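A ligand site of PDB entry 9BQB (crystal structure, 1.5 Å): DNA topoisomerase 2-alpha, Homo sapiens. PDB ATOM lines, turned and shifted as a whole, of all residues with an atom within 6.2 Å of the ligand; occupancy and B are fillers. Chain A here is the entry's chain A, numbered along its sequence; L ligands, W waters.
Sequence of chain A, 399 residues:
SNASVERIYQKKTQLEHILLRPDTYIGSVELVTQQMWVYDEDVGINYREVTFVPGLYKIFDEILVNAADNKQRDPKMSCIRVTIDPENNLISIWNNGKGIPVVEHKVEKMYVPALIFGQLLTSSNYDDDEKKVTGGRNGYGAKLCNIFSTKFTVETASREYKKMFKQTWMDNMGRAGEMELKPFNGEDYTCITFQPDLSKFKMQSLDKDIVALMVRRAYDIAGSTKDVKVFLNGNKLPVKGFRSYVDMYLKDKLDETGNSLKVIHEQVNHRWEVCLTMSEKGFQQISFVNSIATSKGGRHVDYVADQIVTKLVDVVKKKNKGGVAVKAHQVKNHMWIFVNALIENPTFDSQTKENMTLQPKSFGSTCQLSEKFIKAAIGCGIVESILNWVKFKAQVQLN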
ATOM      1  N   VAL A  32      28.841   1.367  21.992  1.00  0.00           N
ATOM      2  CA  VAL A  32      29.639   2.480  21.515  1.00  0.00           C
ATOM      3  C   VAL A  32      29.047   3.741  22.128  1.00  0.00           C
ATOM      4  O   VAL A  32      27.827   3.868  22.245  1.00  0.00           O
ATOM      5  CB  VAL A  32      29.675   2.567  19.971  1.00  0.00           C
ATOM      6  CG1 VAL A  32      29.992   1.210  19.356  1.00  0.00           C
ATOM      7  CG2 VAL A  32      28.378   3.113  19.452  1.00  0.00           C
ATOM      8  N   GLN A  34      29.302   7.762  21.446  1.00  0.00           N
ATOM      9  CA  GLN A  34      29.803   8.777  20.539  1.00  0.00           C
ATOM     10  C   GLN A  34      28.712   9.797  20.283  1.00  0.00           C
ATOM     11  O   GLN A  34      27.539   9.564  20.551  1.00  0.00           O
ATOM     12  CB  GLN A  34      30.276   8.165  19.225  1.00  0.00           C
ATOM     13  CG  GLN A  34      29.159   7.504  18.437  1.00  0.00           C
ATOM     14  CD  GLN A  34      29.667   6.670  17.291  1.00  0.00           C
ATOM     15  OE1 GLN A  34      30.776   6.167  17.342  1.00  0.00           O
ATOM     16  NE2 GLN A  34      28.844   6.501  16.271  1.00  0.00           N
ATOM     17  N   GLN A  35      29.125  10.927  19.730  1.00  0.00           N
ATOM     18  CA  GLN A  35      28.165  11.943  19.351  1.00  0.00           C
ATOM     19  C   GLN A  35      27.476  11.567  18.044  1.00  0.00           C
ATOM     20  O   GLN A  35      28.110  11.128  17.092  1.00  0.00           O
ATOM     21  CB  GLN A  35      28.867  13.287  19.236  1.00  0.00           C
ATOM     22  CG  GLN A  35      29.478  13.680  20.559  1.00  0.00           C
ATOM     23  CD  GLN A  35      29.552  15.148  20.706  1.00  0.00           C
ATOM     24  OE1 GLN A  35      28.571  15.801  21.061  1.00  0.00           O
ATOM     25  NE2 GLN A  35      30.727  15.705  20.424  1.00  0.00           N
ATOM     26  N   MET A  36      26.154  11.752  18.043  1.00  0.00           N
ATOM     27  CA  MET A  36      25.268  11.336  16.970  1.00  0.00           C
ATOM     28  C   MET A  36      24.170  12.379  16.843  1.00  0.00           C
ATOM     29  O   MET A  36      23.868  13.088  17.807  1.00  0.00           O
ATOM     30  CB  MET A  36      24.570   9.985  17.234  1.00  0.00           C
ATOM     31  CG  MET A  36      25.403   8.728  17.393  1.00  0.00           C
ATOM     32  SD  MET A  36      26.147   8.279  15.866  1.00  0.00           S
ATOM     33  CE  MET A  36      24.720   7.489  15.117  1.00  0.00           C
ATOM     34  N   TRP A  37      23.544  12.441  15.673  1.00  0.00           N
ATOM     35  CA  TRP A  37      22.257  13.122  15.533  1.00  0.00           C
ATOM     36  C   TRP A  37      21.127  12.176  15.913  1.00  0.00           C
ATOM     37  O   TRP A  37      21.093  11.024  15.448  1.00  0.00           O
ATOM     38  CB  TRP A  37      22.083  13.610  14.100  1.00  0.00           C
ATOM     39  CG  TRP A  37      23.063  14.656  13.694  1.00  0.00           C
ATOM     40  CD1 TRP A  37      24.234  14.489  12.992  1.00  0.00           C
ATOM     41  CD2 TRP A  37      22.951  16.057  13.965  1.00  0.00           C
ATOM     42  NE1 TRP A  37      24.837  15.708  12.808  1.00  0.00           N
ATOM     43  CE2 TRP A  37      24.079  16.689  13.396  1.00  0.00           C
ATOM     44  CE3 TRP A  37      21.995  16.840  14.617  1.00  0.00           C
ATOM     45  CZ2 TRP A  37      24.270  18.059  13.468  1.00  0.00           C
ATOM     46  CZ3 TRP A  37      22.196  18.208  14.686  1.00  0.00           C
ATOM     47  CH2 TRP A  37      23.316  18.800  14.116  1.00  0.00           C
ATOM     48  N   VAL A  38      20.209  12.641  16.765  1.00  0.00           N
ATOM     49  CA  VAL A  38      19.048  11.893  17.198  1.00  0.00           C
ATOM     50  C   VAL A  38      17.831  12.812  17.138  1.00  0.00           C
ATOM     51  O   VAL A  38      17.956  14.016  16.967  1.00  0.00           O
ATOM     52  CB  VAL A  38      19.211  11.316  18.615  1.00  0.00           C
ATOM     53  CG1 VAL A  38      20.481  10.476  18.730  1.00  0.00           C
ATOM     54  CG2 VAL A  38      19.247  12.432  19.633  1.00  0.00           C
ATOM     55  N   TYR A  47      22.286  17.140  18.219  1.00  0.00           N
ATOM     56  CA  TYR A  47      23.571  16.452  18.228  1.00  0.00           C
ATOM     57  C   TYR A  47      24.029  16.280  19.667  1.00  0.00           C
ATOM     58  O   TYR A  47      24.208  17.278  20.369  1.00  0.00           O
ATOM     59  CB  TYR A  47      24.598  17.246  17.423  1.00  0.00           C
ATOM     60  CG  TYR A  47      25.880  16.519  17.083  1.00  0.00           C
ATOM     61  CD1 TYR A  47      25.879  15.499  16.153  1.00  0.00           C
ATOM     62  CD2 TYR A  47      27.081  16.850  17.697  1.00  0.00           C
ATOM     63  CE1 TYR A  47      27.025  14.815  15.831  1.00  0.00           C
ATOM     64  CE2 TYR A  47      28.255  16.173  17.359  1.00  0.00           C
ATOM     65  CZ  TYR A  47      28.209  15.144  16.427  1.00  0.00           C
ATOM     66  OH  TYR A  47      29.338  14.431  16.068  1.00  0.00           O
ATOM     67  N   PHE A  52      24.905   3.245  22.415  1.00  0.00           N
ATOM     68  CA  PHE A  52      24.035   2.347  21.668  1.00  0.00           C
ATOM     69  C   PHE A  52      24.872   1.217  21.076  1.00  0.00           C
ATOM     70  O   PHE A  52      26.105   1.272  21.027  1.00  0.00           O
ATOM     71  CB  PHE A  52      23.285   3.091  20.548  1.00  0.00           C
ATOM     72  CG  PHE A  52      24.156   3.496  19.386  1.00  0.00           C
ATOM     73  CD1 PHE A  52      25.032   4.564  19.503  1.00  0.00           C
ATOM     74  CD2 PHE A  52      24.106   2.804  18.185  1.00  0.00           C
ATOM     75  CE1 PHE A  52      25.845   4.937  18.443  1.00  0.00           C
ATOM     76  CE2 PHE A  52      24.923   3.169  17.111  1.00  0.00           C
ATOM     77  CZ  PHE A  52      25.793   4.235  17.240  1.00  0.00           C
ATOM     78  N   PRO A  54      25.599  -0.680  17.602  1.00  0.00           N
ATOM     79  CA  PRO A  54      25.366  -0.533  16.150  1.00  0.00           C
ATOM     80  C   PRO A  54      24.559  -1.674  15.534  1.00  0.00           C
ATOM     81  O   PRO A  54      23.683  -1.404  14.694  1.00  0.00           O
ATOM     82  CB  PRO A  54      26.800  -0.455  15.588  1.00  0.00           C
ATOM     83  CG  PRO A  54      27.574   0.216  16.698  1.00  0.00           C
ATOM     84  CD  PRO A  54      27.008  -0.406  17.969  1.00  0.00           C
ATOM     85  N   TYR A  57      20.762  -1.142  15.903  1.00  0.00           N
ATOM     86  CA  TYR A  57      20.315  -0.094  14.986  1.00  0.00           C
ATOM     87  C   TYR A  57      20.248  -0.596  13.559  1.00  0.00           C
ATOM     88  O   TYR A  57      19.316  -0.270  12.807  1.00  0.00           O
ATOM     89  CB  TYR A  57      21.280   1.071  15.090  1.00  0.00           C
ATOM     90  CG  TYR A  57      20.855   2.419  14.559  1.00  0.00           C
ATOM     91  CD1 TYR A  57      19.521   2.781  14.424  1.00  0.00           C
ATOM     92  CD2 TYR A  57      21.813   3.348  14.218  1.00  0.00           C
ATOM     93  CE1 TYR A  57      19.173   4.040  13.952  1.00  0.00           C
ATOM     94  CE2 TYR A  57      21.482   4.597  13.771  1.00  0.00           C
ATOM     95  CZ  TYR A  57      20.162   4.950  13.651  1.00  0.00           C
ATOM     96  OH  TYR A  57      19.876   6.208  13.206  1.00  0.00           O
ATOM     97  N   LEU A 213      17.561   7.347  18.100  1.00  0.00           N
ATOM     98  CA  LEU A 213      18.230   7.063  16.842  1.00  0.00           C
ATOM     99  C   LEU A 213      17.264   6.487  15.814  1.00  0.00           C
ATOM    100  O   LEU A 213      17.321   6.848  14.636  1.00  0.00           O
ATOM    101  CB  LEU A 213      19.377   6.084  17.085  1.00  0.00           C
ATOM    102  CG  LEU A 213      20.646   6.639  17.711  1.00  0.00           C
ATOM    103  CD1 LEU A 213      21.575   5.509  18.191  1.00  0.00           C
ATOM    104  CD2 LEU A 213      21.382   7.529  16.712  1.00  0.00           C
ATOM    105  N   ARG A 216      14.929   9.214  14.570  1.00  0.00           N
ATOM    106  CA  ARG A 216      15.625  10.065  13.601  1.00  0.00           C
ATOM    107  C   ARG A 216      15.740   9.365  12.256  1.00  0.00           C
ATOM    108  O   ARG A 216      15.585   9.987  11.198  1.00  0.00           O
ATOM    109  CB  ARG A 216      17.021  10.474  14.080  1.00  0.00           C
ATOM    110  CG  ARG A 216      17.550  11.719  13.327  1.00  0.00           C
ATOM    111  CD  ARG A 216      19.025  11.624  12.861  1.00  0.00           C
ATOM    112  NE  ARG A 216      19.195  10.532  11.905  1.00  0.00           N
ATOM    113  CZ  ARG A 216      19.916   9.429  12.123  1.00  0.00           C
ATOM    114  NH1 ARG A 216      20.579   9.256  13.269  1.00  0.00           N
ATOM    115  NH2 ARG A 216      19.973   8.502  11.186  1.00  0.00           N
ATOM    116  N   ARG A 217      16.015   8.062  12.266  1.00  0.00           N
ATOM    117  CA  ARG A 217      16.107   7.326  11.002  1.00  0.00           C
ATOM    118  C   ARG A 217      14.793   7.367  10.225  1.00  0.00           C
ATOM    119  O   ARG A 217      14.798   7.437   8.988  1.00  0.00           O
ATOM    120  CB  ARG A 217      16.532   5.879  11.294  1.00  0.00           C
ATOM    121  CG  ARG A 217      17.052   5.151  10.093  1.00  0.00           C
ATOM    122  CD  ARG A 217      18.542   5.546   9.653  1.00  0.00           C
ATOM    123  NE  ARG A 217      18.695   4.783   8.429  1.00  0.00           N
ATOM    124  CZ  ARG A 217      18.428   5.253   7.211  1.00  0.00           C
ATOM    125  NH1 ARG A 217      18.160   6.544   7.032  1.00  0.00           N
ATOM    126  NH2 ARG A 217      18.461   4.420   6.181  1.00  0.00           N
ATOM    127  N   ASP A 220      14.807  10.535   8.502  1.00  0.00           N
ATOM    128  CA  ASP A 220      15.687  10.415   7.339  1.00  0.00           C
ATOM    129  C   ASP A 220      14.918   9.910   6.119  1.00  0.00           C
ATOM    130  O   ASP A 220      15.067  10.421   5.010  1.00  0.00           O
ATOM    131  CB  ASP A 220      16.832   9.413   7.554  1.00  0.00           C
ATOM    132  CG  ASP A 220      17.837   9.761   8.638  1.00  0.00           C
ATOM    133  OD1 ASP A 220      17.825  10.875   9.212  1.00  0.00           O
ATOM    134  OD2 ASP A 220      18.698   8.873   8.867  1.00  0.00           O
ATOM    135  N   TYR A 245      14.016  18.673   5.420  1.00  0.00           N
ATOM    136  CA  TYR A 245      14.745  17.787   6.325  1.00  0.00           C
ATOM    137  C   TYR A 245      16.048  18.443   6.769  1.00  0.00           C
ATOM    138  O   TYR A 245      16.346  18.513   7.972  1.00  0.00           O
ATOM    139  CB  TYR A 245      14.995  16.436   5.631  1.00  0.00           C
ATOM    140  CG  TYR A 245      15.985  15.519   6.338  1.00  0.00           C
ATOM    141  CD1 TYR A 245      15.566  14.675   7.367  1.00  0.00           C
ATOM    142  CD2 TYR A 245      17.329  15.495   5.984  1.00  0.00           C
ATOM    143  CE1 TYR A 245      16.467  13.853   8.009  1.00  0.00           C
ATOM    144  CE2 TYR A 245      18.229  14.672   6.626  1.00  0.00           C
ATOM    145  CZ  TYR A 245      17.799  13.857   7.635  1.00  0.00           C
ATOM    146  OH  TYR A 245      18.711  13.043   8.276  1.00  0.00           O
ATOM    147  N   TYR A 249      18.220  20.431  10.761  1.00  0.00           N
ATOM    148  CA  TYR A 249      19.565  20.494  11.314  1.00  0.00           C
ATOM    149  C   TYR A 249      20.067  21.923  11.454  1.00  0.00           C
ATOM    150  O   TYR A 249      20.823  22.228  12.384  1.00  0.00           O
ATOM    151  CB  TYR A 249      20.539  19.727  10.414  1.00  0.00           C
ATOM    152  CG  TYR A 249      20.359  18.240  10.409  1.00  0.00           C
ATOM    153  CD1 TYR A 249      19.352  17.635   9.664  1.00  0.00           C
ATOM    154  CD2 TYR A 249      21.204  17.432  11.136  1.00  0.00           C
ATOM    155  CE1 TYR A 249      19.187  16.269   9.673  1.00  0.00           C
ATOM    156  CE2 TYR A 249      21.061  16.072  11.141  1.00  0.00           C
ATOM    157  CZ  TYR A 249      20.062  15.495  10.403  1.00  0.00           C
ATOM    158  OH  TYR A 249      19.935  14.124  10.432  1.00  0.00           O
ATOM    159  N   LYS A 281      33.778  22.184  12.837  1.00  0.00           N
ATOM    160  CA  LYS A 281      34.274  20.939  13.427  1.00  0.00           C
ATOM    161  C   LYS A 281      35.088  20.124  12.423  1.00  0.00           C
ATOM    162  O   LYS A 281      35.186  18.898  12.570  1.00  0.00           O
ATOM    163  CB  LYS A 281      33.132  20.046  13.904  1.00  0.00           C
ATOM    164  CG  LYS A 281      31.962  20.705  14.560  1.00  0.00           C
ATOM    165  CD  LYS A 281      30.870  19.665  14.683  1.00  0.00           C
ATOM    166  CE  LYS A 281      29.942  19.937  15.844  1.00  0.00           C
ATOM    167  NZ  LYS A 281      29.666  18.645  16.514  1.00  0.00           N
ATOM    168  N   GLY A 282      35.624  20.747  11.388  1.00  0.00           N
ATOM    169  CA  GLY A 282      36.224  20.022  10.297  1.00  0.00           C
ATOM    170  C   GLY A 282      35.175  19.565   9.308  1.00  0.00           C
ATOM    171  O   GLY A 282      33.979  19.841   9.445  1.00  0.00           O
ATOM    172  N   PHE A 283      35.616  18.858   8.276  1.00  0.00           N
ATOM    173  CA  PHE A 283      34.676  18.438   7.237  1.00  0.00           C
ATOM    174  C   PHE A 283      33.574  17.586   7.847  1.00  0.00           C
ATOM    175  O   PHE A 283      33.844  16.656   8.611  1.00  0.00           O
ATOM    176  CB  PHE A 283      35.390  17.665   6.132  1.00  0.00           C
ATOM    177  CG  PHE A 283      34.456  17.168   5.056  1.00  0.00           C
ATOM    178  CD1 PHE A 283      33.873  18.064   4.170  1.00  0.00           C
ATOM    179  CD2 PHE A 283      34.178  15.820   4.906  1.00  0.00           C
ATOM    180  CE1 PHE A 283      33.016  17.623   3.167  1.00  0.00           C
ATOM    181  CE2 PHE A 283      33.331  15.377   3.900  1.00  0.00           C
ATOM    182  CZ  PHE A 283      32.746  16.278   3.037  1.00  0.00           C
ATOM    183  N   GLN A 284      32.326  17.886   7.485  1.00  0.00           N
ATOM    184  CA  GLN A 284      31.155  17.113   7.901  1.00  0.00           C
ATOM    185  C   GLN A 284      30.306  16.811   6.681  1.00  0.00           C
ATOM    186  O   GLN A 284      30.157  17.662   5.806  1.00  0.00           O
ATOM    187  CB  GLN A 284      30.271  17.864   8.892  1.00  0.00           C
ATOM    188  CG  GLN A 284      30.848  18.205  10.206  1.00  0.00           C
ATOM    189  CD  GLN A 284      29.787  18.793  11.104  1.00  0.00           C
ATOM    190  OE1 GLN A 284      28.891  18.094  11.569  1.00  0.00           O
ATOM    191  NE2 GLN A 284      29.874  20.090  11.321  1.00  0.00           N
ATOM    192  N   GLN A 285      29.709  15.615   6.644  1.00  0.00           N
ATOM    193  CA  GLN A 285      28.814  15.239   5.554  1.00  0.00           C
ATOM    194  C   GLN A 285      27.656  14.432   6.129  1.00  0.00           C
ATOM    195  O   GLN A 285      27.857  13.579   7.000  1.00  0.00           O
ATOM    196  CB  GLN A 285      29.549  14.435   4.466  1.00  0.00           C
ATOM    197  CG  GLN A 285      30.113  13.088   4.927  1.00  0.00           C
ATOM    198  CD  GLN A 285      29.085  11.959   4.874  1.00  0.00           C
ATOM    199  OE1 GLN A 285      28.040  12.075   4.224  1.00  0.00           O
ATOM    200  NE2 GLN A 285      29.375  10.873   5.559  1.00  0.00           N
ATOM    201  N   ILE A 286      26.451  14.735   5.668  1.00  0.00           N
ATOM    202  CA  ILE A 286      25.249  13.930   5.909  1.00  0.00           C
ATOM    203  C   ILE A 286      24.754  13.521   4.528  1.00  0.00           C
ATOM    204  O   ILE A 286      24.490  14.383   3.686  1.00  0.00           O
ATOM    205  CB  ILE A 286      24.176  14.697   6.705  1.00  0.00           C
ATOM    206  CG1 ILE A 286      24.625  14.830   8.170  1.00  0.00           C
ATOM    207  CG2 ILE A 286      22.847  14.005   6.592  1.00  0.00           C
ATOM    208  CD1 ILE A 286      23.699  15.578   9.095  1.00  0.00           C
ATOM    209  N   SER A 287      24.695  12.216   4.268  1.00  0.00           N
ATOM    210  CA  SER A 287      24.404  11.768   2.907  1.00  0.00           C
ATOM    211  C   SER A 287      23.641  10.456   2.919  1.00  0.00           C
ATOM    212  O   SER A 287      23.691   9.674   3.876  1.00  0.00           O
ATOM    213  CB  SER A 287      25.689  11.636   2.078  1.00  0.00           C
ATOM    214  OG  SER A 287      26.550  10.629   2.605  1.00  0.00           O
ATOM    215  N   PHE A 288      22.936  10.227   1.804  1.00  0.00           N
ATOM    216  CA  PHE A 288      22.099   9.049   1.576  1.00  0.00           C
ATOM    217  C   PHE A 288      22.327   8.573   0.155  1.00  0.00           C
ATOM    218  O   PHE A 288      22.417   9.375  -0.779  1.00  0.00           O
ATOM    219  CB  PHE A 288      20.598   9.374   1.799  1.00  0.00           C
ATOM    220  CG  PHE A 288      20.346   9.958   3.153  1.00  0.00           C
ATOM    221  CD1 PHE A 288      20.139   9.145   4.255  1.00  0.00           C
ATOM    222  CD2 PHE A 288      20.420  11.327   3.354  1.00  0.00           C
ATOM    223  CE1 PHE A 288      19.978   9.674   5.524  1.00  0.00           C
ATOM    224  CE2 PHE A 288      20.261  11.865   4.625  1.00  0.00           C
ATOM    225  CZ  PHE A 288      20.043  11.027   5.710  1.00  0.00           C
ATOM    226  N   ALA A 293      21.699   5.503   4.884  1.00  0.00           N
ATOM    227  CA  ALA A 293      22.537   6.554   5.483  1.00  0.00           C
ATOM    228  C   ALA A 293      24.015   6.154   5.328  1.00  0.00           C
ATOM    229  O   ALA A 293      24.478   5.214   5.972  1.00  0.00           O
ATOM    230  CB  ALA A 293      22.191   6.761   6.955  1.00  0.00           C
ATOM    231  N   THR A 294      24.746   6.881   4.472  1.00  0.00           N
ATOM    232  CA  THR A 294      26.152   6.555   4.187  1.00  0.00           C
ATOM    233  C   THR A 294      27.037   7.366   5.129  1.00  0.00           C
ATOM    234  O   THR A 294      27.644   8.381   4.779  1.00  0.00           O
ATOM    235  CB  THR A 294      26.481   6.781   2.709  1.00  0.00           C
ATOM    236  OG1 THR A 294      25.954   8.033   2.249  1.00  0.00           O
ATOM    237  CG2 THR A 294      25.902   5.659   1.865  1.00  0.00           C
ATOM    238  N   SER A 295      27.118   6.887   6.372  1.00  0.00           N
ATOM    239  CA  SER A 295      27.747   7.674   7.429  1.00  0.00           C
ATOM    240  C   SER A 295      29.263   7.718   7.334  1.00  0.00           C
ATOM    241  O   SER A 295      29.870   8.570   7.994  1.00  0.00           O
ATOM    242  CB  SER A 295      27.340   7.143   8.806  1.00  0.00           C
ATOM    243  OG  SER A 295      27.564   5.772   8.927  1.00  0.00           O
ATOM    244  N   LYS A 296      29.893   6.867   6.541  1.00  0.00           N
ATOM    245  CA  LYS A 296      31.312   7.017   6.256  1.00  0.00           C
ATOM    246  C   LYS A 296      31.565   7.715   4.931  1.00  0.00           C
ATOM    247  O   LYS A 296      32.728   7.971   4.587  1.00  0.00           O
ATOM    248  CB  LYS A 296      32.016   5.652   6.306  1.00  0.00           C
ATOM    249  CG  LYS A 296      32.159   5.121   7.733  1.00  0.00           C
ATOM    250  CD  LYS A 296      32.727   3.715   7.751  1.00  0.00           C
ATOM    251  CE  LYS A 296      32.819   3.129   9.152  1.00  0.00           C
ATOM    252  NZ  LYS A 296      33.565   4.021  10.049  1.00  0.00           N
ATOM    253  N   GLY A 297      30.512   8.059   4.194  1.00  0.00           N
ATOM    254  CA  GLY A 297      30.616   8.814   2.971  1.00  0.00           C
ATOM    255  C   GLY A 297      30.726   7.924   1.749  1.00  0.00           C
ATOM    256  O   GLY A 297      30.032   6.913   1.635  1.00  0.00           O
ATOM    257  N   GLU A 354      27.896   1.701   4.858  1.00  0.00           N
ATOM    258  CA  GLU A 354      28.237   3.031   5.344  1.00  0.00           C
ATOM    259  C   GLU A 354      29.133   3.810   4.406  1.00  0.00           C
ATOM    260  O   GLU A 354      29.127   5.042   4.475  1.00  0.00           O
ATOM    261  CB  GLU A 354      28.899   2.906   6.723  1.00  0.00           C
ATOM    262  CG  GLU A 354      27.910   2.332   7.752  1.00  0.00           C
ATOM    263  CD  GLU A 354      28.510   2.038   9.103  1.00  0.00           C
ATOM    264  OE1 GLU A 354      29.740   2.059   9.228  1.00  0.00           O
ATOM    265  OE2 GLU A 354      27.735   1.780  10.049  1.00  0.00           O
HETATM  266  C1  LIG L   1      33.261  15.790  13.604  1.00  0.00           C
HETATM  267  C2  LIG L   1      30.827  12.885  12.963  1.00  0.00           C
HETATM  268  C3  LIG L   1      28.353  12.928  12.852  1.00  0.00           C
HETATM  269  C4  LIG L   1      25.383   9.457  12.070  1.00  0.00           C
HETATM  270  C5  LIG L   1      24.443  10.719   9.585  1.00  0.00           C
HETATM  271  C6  LIG L   1      27.239   7.411  12.405  1.00  0.00           C
HETATM  272  C7  LIG L   1      25.038   8.098  11.782  1.00  0.00           C
HETATM  273  C8  LIG L   1      26.664   9.779  12.508  1.00  0.00           C
HETATM  274  C9  LIG L   1      25.950   7.073  11.952  1.00  0.00           C
HETATM  275  C10 LIG L   1      23.658  10.253   8.523  1.00  0.00           C
HETATM  276  C11 LIG L   1      23.308   6.607  11.090  1.00  0.00           C
HETATM  277  C12 LIG L   1      25.783  10.987   9.383  1.00  0.00           C
HETATM  278  C13 LIG L   1      28.223  11.475  13.246  1.00  0.00           C
HETATM  279  N1  LIG L   1      29.579  13.580  13.392  1.00  0.00           N
HETATM  280  C14 LIG L   1      24.270  10.493  12.064  1.00  0.00           C
HETATM  281  O1  LIG L   1      26.931  11.086  12.746  1.00  0.00           O
HETATM  282  C15 LIG L   1      24.229   5.518  11.292  1.00  0.00           C
HETATM  283  C16 LIG L   1      24.208  10.048   7.247  1.00  0.00           C
HETATM  284  C17 LIG L   1      26.415   4.579  11.913  1.00  0.00           C
HETATM  285  C18 LIG L   1      30.790  15.756  13.414  1.00  0.00           C
HETATM  286  C19 LIG L   1      22.468  11.636  10.866  1.00  0.00           C
HETATM  287  C20 LIG L   1      29.618  15.036  12.914  1.00  0.00           C
HETATM  288  C21 LIG L   1      26.400   4.156  13.417  1.00  0.00           C
HETATM  289  C22 LIG L   1      25.578  10.295   7.051  1.00  0.00           C
HETATM  290  C23 LIG L   1      22.198  10.061   8.805  1.00  0.00           C
HETATM  291  C24 LIG L   1      27.214   2.897  13.646  1.00  0.00           C
HETATM  292  C25 LIG L   1      21.721  11.373   9.513  1.00  0.00           C
HETATM  293  C26 LIG L   1      31.993  13.622  13.567  1.00  0.00           C
HETATM  294  C27 LIG L   1      26.369  10.793   8.111  1.00  0.00           C
HETATM  295  C28 LIG L   1      27.602   8.739  12.667  1.00  0.00           C
HETATM  296  C29 LIG L   1      25.489   5.711  11.672  1.00  0.00           C
HETATM  297  N2  LIG L   1      23.783  10.937  10.842  1.00  0.00           N
HETATM  298  N3  LIG L   1      32.043  15.043  13.010  1.00  0.00           N
HETATM  299  O2  LIG L   1      23.711   7.900  11.364  1.00  0.00           O
HETATM  300  O3  LIG L   1      23.802  10.867  13.136  1.00  0.00           O
HETATM  301  O4  LIG L   1      22.139   6.460  10.766  1.00  0.00           O
HETATM  302  O   HOH W   1      28.103  13.840   9.636  1.00  0.00           O
HETATM  303  O   HOH W   2      21.534   3.815   9.692  1.00  0.00           O
HETATM  304  O   HOH W   3      25.177   4.519   8.576  1.00  0.00           O
HETATM  305  O   HOH W   4      32.696  14.728  10.346  1.00  0.00           O
HETATM  306  O   HOH W   5      35.667  17.596  15.272  1.00  0.00           O
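A nitrogen (N1) of the ligand sits close to the side-chain hydroxyl (OH) of Tyr 47.
O3 of the ligand sits at hydrogen-bond distance from N of Trp 37, 3.0 Å away.
The guanidinium group (NH2) of Arg 216 sits at hydrogen-bond distance from an oxygen (O4) of the ligand, at 3.0 Å.
An oxygen (O4) of the ligand lies within hydrogen-bond range of the side-chain hydroxyl (OH) of Tyr 57.
Merely in contact with the ligand: Gln 35 (3.9 Å), Met 36 (3.4 Å), Phe 52 (3.9 Å), Pro 54 (3.9 Å), Arg 217 (3.9 Å), Asp 220 (3.7 Å), Tyr 245 (3.7 Å), Tyr 249 (3.4 Å), Lys 281 (3.8 Å), Gln 284 (3.4 Å), Gln 285 (3.3 Å), Ile 286 (3.8 Å), Ser 287 (3.4 Å), Phe 288 (3.9 Å), Ala 293 (3.8 Å), Thr 294 (3.6 Å), Ser 295 (3.4 Å) and Glu 354 (3.6 Å).
Within 4 Å of the ligand: Gln 35, Met 36, Trp 37, Tyr 47, Phe 52, Pro 54, Tyr 57, Arg 216, Arg 217, Asp 220, Tyr 245, Tyr 249, Lys 281, Gln 284, Gln 285, Ile 286, Ser 287, Phe 288, Ala 293, Thr 294, Ser 295 and Glu 354.
The nearest printed residue that does not touch the ligand is Gln 34 (4.3 Å).
The guanidinium group of Arg 216 is in hydrogen-bond range of the backbone carbonyl oxygen of Trp 37 (2.9 Å).
The guanidinium group (NH2) of Arg 216 lies within hydrogen-bond range of the side-chain hydroxyl (OH) of Tyr 57, 3.1 Å away.
The side-chain carboxylate (OD2) of Asp 220 lies within salt-bridge range of the guanidinium group (NH2) of Arg 216.
OH of Tyr 57 is in hydrogen-bond range of O of Leu 213 (3.0 Å).
OE1 of Gln 285 is in hydrogen-bond range of OG of Ser 287 (2.6 Å).
The side-chain amide nitrogen (NE2) of Gln 285 lies within hydrogen-bond range of the backbone carbonyl oxygen (O) of Thr 294 (3.1 Å).
The side-chain hydroxyl (OH) of Tyr 245 lies within hydrogen-bond range of the side-chain hydroxyl (OH) of Tyr 249 (2.7 Å).
N of Lys 296 is in hydrogen-bond range of O of Glu 354, at 2.9 Å.
Water W2 bridges an oxygen (O4) of the ligand (2.9 Å) and the guanidinium group (NE) of Arg 217 (3.3 Å).
Water W3 lies within hydrogen-bond range of the side-chain hydroxyl of Ser 295 (2.7 Å) and the backbone carbonyl oxygen of Ala 293 (2.8 Å).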
